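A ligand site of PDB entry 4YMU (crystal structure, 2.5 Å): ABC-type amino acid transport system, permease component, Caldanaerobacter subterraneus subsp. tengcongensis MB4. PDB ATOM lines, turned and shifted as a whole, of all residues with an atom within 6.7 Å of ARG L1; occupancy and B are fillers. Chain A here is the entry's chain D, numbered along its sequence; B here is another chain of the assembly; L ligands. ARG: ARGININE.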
ATOM      1  N   ILE A  62      12.514  -1.993  -4.525  1.00  0.00           N
ATOM      2  CA  ILE A  62      12.559  -0.895  -5.497  1.00  0.00           C
ATOM      3  C   ILE A  62      12.856  -1.349  -6.924  1.00  0.00           C
ATOM      4  O   ILE A  62      12.238  -0.861  -7.876  1.00  0.00           O
ATOM      5  CB  ILE A  62      13.516   0.184  -5.033  1.00  0.00           C
ATOM      6  CG1 ILE A  62      12.942   0.821  -3.775  1.00  0.00           C
ATOM      7  CG2 ILE A  62      13.696   1.239  -6.104  1.00  0.00           C
ATOM      8  CD1 ILE A  62      13.856   1.767  -3.158  1.00  0.00           C
ATOM      9  N   ARG A  63      13.785  -2.283  -7.094  1.00  0.00           N
ATOM     10  CA  ARG A  63      14.102  -2.746  -8.428  1.00  0.00           C
ATOM     11  C   ARG A  63      13.024  -3.680  -8.960  1.00  0.00           C
ATOM     12  O   ARG A  63      12.810  -3.785 -10.172  1.00  0.00           O
ATOM     13  CB  ARG A  63      15.468  -3.445  -8.439  1.00  0.00           C
ATOM     14  CG  ARG A  63      16.621  -2.540  -8.046  1.00  0.00           C
ATOM     15  CD  ARG A  63      17.947  -3.291  -8.072  1.00  0.00           C
ATOM     16  NE  ARG A  63      18.300  -3.759  -9.399  1.00  0.00           N
ATOM     17  CZ  ARG A  63      18.592  -5.022  -9.677  1.00  0.00           C
ATOM     18  NH1 ARG A  63      18.560  -5.928  -8.708  1.00  0.00           N
ATOM     19  NH2 ARG A  63      18.899  -5.380 -10.921  1.00  0.00           N
ATOM     20  N   GLY A  64      12.326  -4.344  -8.041  1.00  0.00           N
ATOM     21  CA  GLY A  64      11.347  -5.347  -8.431  1.00  0.00           C
ATOM     22  C   GLY A  64       9.957  -4.758  -8.617  1.00  0.00           C
ATOM     23  O   GLY A  64       8.975  -5.512  -8.747  1.00  0.00           O
ATOM     24  N   THR A  65       9.887  -3.429  -8.687  1.00  0.00           N
ATOM     25  CA  THR A  65       8.614  -2.719  -8.669  1.00  0.00           C
ATOM     26  C   THR A  65       8.666  -1.473  -9.595  1.00  0.00           C
ATOM     27  O   THR A  65       9.692  -0.805  -9.682  1.00  0.00           O
ATOM     28  CB  THR A  65       8.282  -2.359  -7.194  1.00  0.00           C
ATOM     29  OG1 THR A  65       6.895  -2.593  -6.925  1.00  0.00           O
ATOM     30  CG2 THR A  65       8.689  -0.948  -6.836  1.00  0.00           C
ATOM     31  N   PRO A  66       7.574  -1.186 -10.330  1.00  0.00           N
ATOM     32  CA  PRO A  66       7.630  -0.158 -11.380  1.00  0.00           C
ATOM     33  C   PRO A  66       7.921   1.268 -10.885  1.00  0.00           C
ATOM     34  O   PRO A  66       7.454   1.679  -9.807  1.00  0.00           O
ATOM     35  CB  PRO A  66       6.235  -0.218 -12.015  1.00  0.00           C
ATOM     36  CG  PRO A  66       5.728  -1.584 -11.702  1.00  0.00           C
ATOM     37  CD  PRO A  66       6.269  -1.872 -10.323  1.00  0.00           C
ATOM     38  N   LEU A  67       8.717   2.011 -11.665  1.00  0.00           N
ATOM     39  CA  LEU A  67       9.046   3.406 -11.370  1.00  0.00           C
ATOM     40  C   LEU A  67       7.758   4.249 -11.286  1.00  0.00           C
ATOM     41  O   LEU A  67       7.656   5.134 -10.451  1.00  0.00           O
ATOM     42  CB  LEU A  67       9.951   3.976 -12.456  1.00  0.00           C
ATOM     43  CG  LEU A  67      10.943   5.117 -12.177  1.00  0.00           C
ATOM     44  CD1 LEU A  67      11.014   6.085 -13.349  1.00  0.00           C
ATOM     45  CD2 LEU A  67      10.734   5.846 -10.867  1.00  0.00           C
ATOM     46  N   LEU A  68       6.813   3.993 -12.190  1.00  0.00           N
ATOM     47  CA  LEU A  68       5.553   4.734 -12.240  1.00  0.00           C
ATOM     48  C   LEU A  68       4.866   4.649 -10.890  1.00  0.00           C
ATOM     49  O   LEU A  68       4.539   5.692 -10.271  1.00  0.00           O
ATOM     50  CB  LEU A  68       4.610   4.156 -13.306  1.00  0.00           C
ATOM     51  CG  LEU A  68       3.688   5.061 -14.131  1.00  0.00           C
ATOM     52  CD1 LEU A  68       2.408   4.320 -14.503  1.00  0.00           C
ATOM     53  CD2 LEU A  68       3.384   6.393 -13.458  1.00  0.00           C
ATOM     54  N   GLN A  70       6.016   4.067  -8.030  1.00  0.00           N
ATOM     55  CA  GLN A  70       6.745   4.807  -7.014  1.00  0.00           C
ATOM     56  C   GLN A  70       6.464   6.305  -7.122  1.00  0.00           C
ATOM     57  O   GLN A  70       6.268   6.991  -6.099  1.00  0.00           O
ATOM     58  CB  GLN A  70       8.250   4.533  -7.109  1.00  0.00           C
ATOM     59  CG  GLN A  70       8.634   3.098  -6.796  1.00  0.00           C
ATOM     60  CD  GLN A  70      10.008   2.673  -7.369  1.00  0.00           C
ATOM     61  OE1 GLN A  70      10.217   1.506  -7.708  1.00  0.00           O
ATOM     62  NE2 GLN A  70      10.926   3.620  -7.470  1.00  0.00           N
ATOM     63  N   LEU A  95      12.718   9.342  -8.725  1.00  0.00           N
ATOM     64  CA  LEU A  95      13.834   8.974  -9.578  1.00  0.00           C
ATOM     65  C   LEU A  95      15.112   8.715  -8.757  1.00  0.00           C
ATOM     66  O   LEU A  95      15.811   7.737  -8.998  1.00  0.00           O
ATOM     67  CB  LEU A  95      14.101  10.075 -10.594  1.00  0.00           C
ATOM     68  CG  LEU A  95      13.061  10.273 -11.693  1.00  0.00           C
ATOM     69  CD1 LEU A  95      13.573  11.256 -12.704  1.00  0.00           C
ATOM     70  CD2 LEU A  95      12.753   8.956 -12.352  1.00  0.00           C
ATOM     71  N   ASN A  98      14.621   5.281  -6.933  1.00  0.00           N
ATOM     72  CA  ASN A  98      14.746   4.202  -7.923  1.00  0.00           C
ATOM     73  C   ASN A  98      16.221   3.974  -8.293  1.00  0.00           C
ATOM     74  O   ASN A  98      16.797   2.864  -8.168  1.00  0.00           O
ATOM     75  CB  ASN A  98      13.886   4.558  -9.140  1.00  0.00           C
ATOM     76  CG  ASN A  98      13.851   3.466 -10.185  1.00  0.00           C
ATOM     77  OD1 ASN A  98      14.516   3.572 -11.227  1.00  0.00           O
ATOM     78  ND2 ASN A  98      13.083   2.409  -9.934  1.00  0.00           N
ATOM     79  N   SER A  99      16.856   5.078  -8.693  1.00  0.00           N
ATOM     80  CA  SER A  99      18.253   5.088  -9.049  1.00  0.00           C
ATOM     81  C   SER A  99      19.097   4.640  -7.885  1.00  0.00           C
ATOM     82  O   SER A  99      20.123   4.023  -8.097  1.00  0.00           O
ATOM     83  CB  SER A  99      18.696   6.482  -9.509  1.00  0.00           C
ATOM     84  OG  SER A  99      20.052   6.442  -9.921  1.00  0.00           O
ATOM     85  N   SER A 100      18.697   4.953  -6.660  1.00  0.00           N
ATOM     86  CA  SER A 100      19.525   4.561  -5.509  1.00  0.00           C
ATOM     87  C   SER A 100      19.607   3.049  -5.460  1.00  0.00           C
ATOM     88  O   SER A 100      20.687   2.474  -5.230  1.00  0.00           O
ATOM     89  CB  SER A 100      18.969   5.099  -4.198  1.00  0.00           C
ATOM     90  OG  SER A 100      17.919   4.280  -3.713  1.00  0.00           O
ATOM     91  N   ALA A 101      18.475   2.382  -5.671  1.00  0.00           N
ATOM     92  CA  ALA A 101      18.512   0.925  -5.664  1.00  0.00           C
ATOM     93  C   ALA A 101      19.443   0.385  -6.765  1.00  0.00           C
ATOM     94  O   ALA A 101      20.374  -0.444  -6.513  1.00  0.00           O
ATOM     95  CB  ALA A 101      17.124   0.352  -5.800  1.00  0.00           C
ATOM     96  N   TYR A 102      19.207   0.839  -7.995  1.00  0.00           N
ATOM     97  CA  TYR A 102      20.009   0.315  -9.098  1.00  0.00           C
ATOM     98  C   TYR A 102      21.514   0.602  -8.929  1.00  0.00           C
ATOM     99  O   TYR A 102      22.355  -0.241  -9.238  1.00  0.00           O
ATOM    100  CB  TYR A 102      19.484   0.808 -10.456  1.00  0.00           C
ATOM    101  CG  TYR A 102      18.153   0.186 -10.823  1.00  0.00           C
ATOM    102  CD1 TYR A 102      18.104  -1.005 -11.551  1.00  0.00           C
ATOM    103  CD2 TYR A 102      16.949   0.771 -10.442  1.00  0.00           C
ATOM    104  CE1 TYR A 102      16.880  -1.581 -11.884  1.00  0.00           C
ATOM    105  CE2 TYR A 102      15.720   0.202 -10.770  1.00  0.00           C
ATOM    106  CZ  TYR A 102      15.694  -0.974 -11.492  1.00  0.00           C
ATOM    107  OH  TYR A 102      14.475  -1.543 -11.829  1.00  0.00           O
ATOM    108  N   VAL A 103      21.824   1.779  -8.379  1.00  0.00           N
ATOM    109  CA  VAL A 103      23.203   2.179  -8.120  1.00  0.00           C
ATOM    110  C   VAL A 103      23.858   1.321  -7.030  1.00  0.00           C
ATOM    111  O   VAL A 103      25.037   0.949  -7.145  1.00  0.00           O
ATOM    112  CB  VAL A 103      23.300   3.670  -7.787  1.00  0.00           C
ATOM    113  CG1 VAL A 103      24.600   4.008  -7.069  1.00  0.00           C
ATOM    114  CG2 VAL A 103      23.162   4.483  -9.076  1.00  0.00           C
ATOM    115  N   GLU A 152      23.945   4.503 -16.182  1.00  0.00           N
ATOM    116  CA  GLU A 152      22.734   4.663 -15.413  1.00  0.00           C
ATOM    117  C   GLU A 152      22.069   5.980 -15.774  1.00  0.00           C
ATOM    118  O   GLU A 152      20.882   6.020 -16.058  1.00  0.00           O
ATOM    119  CB  GLU A 152      23.039   4.568 -13.911  1.00  0.00           C
ATOM    120  CG  GLU A 152      21.959   5.133 -12.987  1.00  0.00           C
ATOM    121  CD  GLU A 152      20.723   4.243 -12.848  1.00  0.00           C
ATOM    122  OE1 GLU A 152      20.537   3.288 -13.643  1.00  0.00           O
ATOM    123  OE2 GLU A 152      19.928   4.509 -11.910  1.00  0.00           O
ATOM    124  N   VAL A 155      20.265   5.949 -19.077  1.00  0.00           N
ATOM    125  CA  VAL A 155      19.003   5.234 -18.944  1.00  0.00           C
ATOM    126  C   VAL A 155      17.953   6.110 -18.246  1.00  0.00           C
ATOM    127  O   VAL A 155      16.771   6.138 -18.630  1.00  0.00           O
ATOM    128  CB  VAL A 155      19.182   3.937 -18.138  1.00  0.00           C
ATOM    129  CG1 VAL A 155      17.844   3.314 -17.812  1.00  0.00           C
ATOM    130  CG2 VAL A 155      20.025   2.962 -18.928  1.00  0.00           C
ATOM    131  N   MET A 156      18.408   6.852 -17.232  1.00  0.00           N
ATOM    132  CA  MET A 156      17.517   7.690 -16.451  1.00  0.00           C
ATOM    133  C   MET A 156      16.962   8.872 -17.229  1.00  0.00           C
ATOM    134  O   MET A 156      15.922   9.394 -16.863  1.00  0.00           O
ATOM    135  CB  MET A 156      18.241   8.170 -15.190  1.00  0.00           C
ATOM    136  CG  MET A 156      18.375   7.107 -14.127  1.00  0.00           C
ATOM    137  SD  MET A 156      16.766   6.614 -13.451  1.00  0.00           S
ATOM    138  CE  MET A 156      16.601   7.877 -12.193  1.00  0.00           C
ATOM    139  N   GLU A 159      14.122   7.448 -18.618  1.00  0.00           N
ATOM    140  CA  GLU A 159      13.205   7.168 -17.514  1.00  0.00           C
ATOM    141  C   GLU A 159      12.432   8.399 -17.015  1.00  0.00           C
ATOM    142  O   GLU A 159      11.272   8.279 -16.633  1.00  0.00           O
ATOM    143  CB  GLU A 159      13.937   6.475 -16.362  1.00  0.00           C
ATOM    144  CG  GLU A 159      14.331   5.026 -16.678  1.00  0.00           C
ATOM    145  CD  GLU A 159      13.145   4.101 -16.860  1.00  0.00           C
ATOM    146  OE1 GLU A 159      12.048   4.420 -16.382  1.00  0.00           O
ATOM    147  OE2 GLU A 159      13.308   3.016 -17.459  1.00  0.00           O
ATOM    148  N   ILE A 162       8.802  10.174 -17.517  1.00  0.00           N
ATOM    149  CA  ILE A 162       7.600   9.734 -16.828  1.00  0.00           C
ATOM    150  C   ILE A 162       7.043  10.773 -15.856  1.00  0.00           C
ATOM    151  O   ILE A 162       5.914  10.638 -15.380  1.00  0.00           O
ATOM    152  CB  ILE A 162       7.837   8.406 -16.118  1.00  0.00           C
ATOM    153  CG1 ILE A 162       6.551   7.593 -16.099  1.00  0.00           C
ATOM    154  CG2 ILE A 162       8.436   8.615 -14.707  1.00  0.00           C
ATOM    155  CD1 ILE A 162       6.662   6.433 -15.191  1.00  0.00           C
ATOM    156  N   VAL B 155      10.834  -7.733 -17.221  1.00  0.00           N
ATOM    157  CA  VAL B 155      11.035  -6.286 -17.316  1.00  0.00           C
ATOM    158  C   VAL B 155       9.782  -5.613 -17.866  1.00  0.00           C
ATOM    159  O   VAL B 155       9.360  -4.551 -17.379  1.00  0.00           O
ATOM    160  CB  VAL B 155      12.248  -5.955 -18.206  1.00  0.00           C
ATOM    161  CG1 VAL B 155      12.278  -4.474 -18.552  1.00  0.00           C
ATOM    162  CG2 VAL B 155      13.519  -6.382 -17.527  1.00  0.00           C
ATOM    163  N   LYS B 158       6.813  -4.676 -15.455  1.00  0.00           N
ATOM    164  CA  LYS B 158       6.966  -3.351 -14.856  1.00  0.00           C
ATOM    165  C   LYS B 158       6.685  -2.273 -15.877  1.00  0.00           C
ATOM    166  O   LYS B 158       5.981  -1.304 -15.590  1.00  0.00           O
ATOM    167  CB  LYS B 158       8.353  -3.177 -14.243  1.00  0.00           C
ATOM    168  CG  LYS B 158       8.611  -4.117 -13.093  1.00  0.00           C
ATOM    169  CD  LYS B 158       9.863  -3.732 -12.329  1.00  0.00           C
ATOM    170  CE  LYS B 158      11.112  -3.924 -13.174  1.00  0.00           C
ATOM    171  NZ  LYS B 158      12.297  -3.242 -12.545  1.00  0.00           N
ATOM    172  N   GLU B 159       7.211  -2.468 -17.085  1.00  0.00           N
ATOM    173  CA  GLU B 159       7.075  -1.482 -18.145  1.00  0.00           C
ATOM    174  C   GLU B 159       5.598  -1.213 -18.475  1.00  0.00           C
ATOM    175  O   GLU B 159       5.218  -0.070 -18.730  1.00  0.00           O
ATOM    176  CB  GLU B 159       7.802  -1.985 -19.397  1.00  0.00           C
ATOM    177  CG  GLU B 159       9.321  -1.987 -19.263  1.00  0.00           C
ATOM    178  CD  GLU B 159       9.910  -0.591 -19.187  1.00  0.00           C
ATOM    179  OE1 GLU B 159       9.257   0.361 -19.662  1.00  0.00           O
ATOM    180  OE2 GLU B 159      11.004  -0.421 -18.627  1.00  0.00           O
HETATM  181  N   ARG L   1      11.218   1.376 -16.376  1.00  0.00           N
HETATM  182  CA  ARG L   1      11.619   0.223 -15.563  1.00  0.00           C
HETATM  183  C   ARG L   1      10.911   0.201 -14.221  1.00  0.00           C
HETATM  184  O   ARG L   1      11.014  -0.793 -13.487  1.00  0.00           O
HETATM  185  CB  ARG L   1      13.124   0.233 -15.320  1.00  0.00           C
HETATM  186  CG  ARG L   1      13.605   1.317 -14.379  1.00  0.00           C
HETATM  187  CD  ARG L   1      15.126   1.346 -14.385  1.00  0.00           C
HETATM  188  NE  ARG L   1      15.665   2.219 -13.356  1.00  0.00           N
HETATM  189  CZ  ARG L   1      16.941   2.591 -13.290  1.00  0.00           C
HETATM  190  NH1 ARG L   1      17.349   3.388 -12.301  1.00  0.00           N
HETATM  191  NH2 ARG L   1      17.807   2.164 -14.194  1.00  0.00           N
HETATM  192  OXT ARG L   1      10.244   1.164 -13.845  1.00  0.00           O
HETATM  193  N   ARG L   2      11.664   2.543 -19.570  1.00  0.00           N
HETATM  194  CA  ARG L   2      12.833   2.617 -20.441  1.00  0.00           C
HETATM  195  C   ARG L   2      12.511   3.358 -21.733  1.00  0.00           C
HETATM  196  O   ARG L   2      13.430   3.780 -22.444  1.00  0.00           O
HETATM  197  CB  ARG L   2      13.356   1.216 -20.782  1.00  0.00           C
HETATM  198  CG  ARG L   2      12.451   0.410 -21.700  1.00  0.00           C
HETATM  199  CD  ARG L   2      12.922  -1.019 -21.800  1.00  0.00           C
HETATM  200  NE  ARG L   2      12.231  -1.771 -22.838  1.00  0.00           N
HETATM  201  CZ  ARG L   2      12.336  -3.087 -23.007  1.00  0.00           C
HETATM  202  NH1 ARG L   2      13.115  -3.792 -22.188  1.00  0.00           N
HETATM  203  NH2 ARG L   2      11.679  -3.704 -23.970  1.00  0.00           N
HETATM  204  OXT ARG L   2      11.336   3.542 -22.099  1.00  0.00           O
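SD of Met 156 sits at hydrogen-bond distance from NH1 of ARG L1 (3.5 Å).
The side-chain carboxylate (OE2) of Glu 159 of chain A is in salt-bridge range of a nitrogen (N) of ARG L1, 2.9 Å away.
N of Leu 67 sits at hydrogen-bond distance from OXT of ARG L1 (2.8 Å).
N of ARG L2 lies within salt-bridge range of OE2 of Glu 159 of chain B (3.2 Å).
A nitrogen (N) of ARG L1 lies within salt-bridge range of the side-chain carboxylate (OE2) of Glu 159 of chain B (2.9 Å).
The side-chain amino group (NZ) of Lys 158 of chain B is in salt-bridge range of an oxygen (O) of ARG L1 (2.9 Å).
A nitrogen (N) of ARG L2 lies within salt-bridge range of the side-chain carboxylate (OE2) of Glu 159 of chain A.
The side-chain amide oxygen of Asn 98 is in hydrogen-bond range of a nitrogen (NE) of ARG L1 (2.8 Å).
The side-chain carboxylate of Glu 152 is in salt-bridge range of a nitrogen (NH1) of ARG L1 (2.8 Å).
N of ARG L2 sits close to N of ARG L1 (3.4 Å).
O of Arg 63 lies within hydrogen-bond range of OH of Tyr 102 (3.2 Å).
The side-chain amide nitrogen (NE2) of Gln 70 sits close to the side-chain amide nitrogen (ND2) of Asn 98 (3.5 Å).
The side-chain carboxylate (OE2) of Glu 152 is in hydrogen-bond range of the side-chain hydroxyl (OG) of Ser 99, 2.8 Å away.
The backbone carbonyl oxygen (O) of Pro 66 lies close to the side-chain amide oxygen (OE1) of Gln 70 (3.5 Å).
The side-chain amino group (NZ) of Lys 158 of chain B sits at hydrogen-bond distance from the backbone carbonyl oxygen (O) of Arg 63, at 2.5 Å.
OH of Tyr 102 sits at hydrogen-bond distance from NZ of Lys 158 of chain B, 2.9 Å away.
Merely in contact with ARG L1: Tyr 102 (3.2 Å), Pro 66 (3.8 Å), Ser 99 (3.8 Å) and Val 155 of chain A (3.8 Å).
11 residues have an atom within 4 Å of ARG L1: Pro 66, Leu 67, Asn 98, Ser 99, Tyr 102, Glu 152, Val 155 of chain A, Met 156, Glu 159 of chain A, Lys 158 of chain B and Glu 159 of chain B.
Along chain A the residues within 4 Å of ARG L1 span positions 66 to 159.
The nearest printed residue that does not touch ARG L1 is Thr 65 (4.03 Å).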
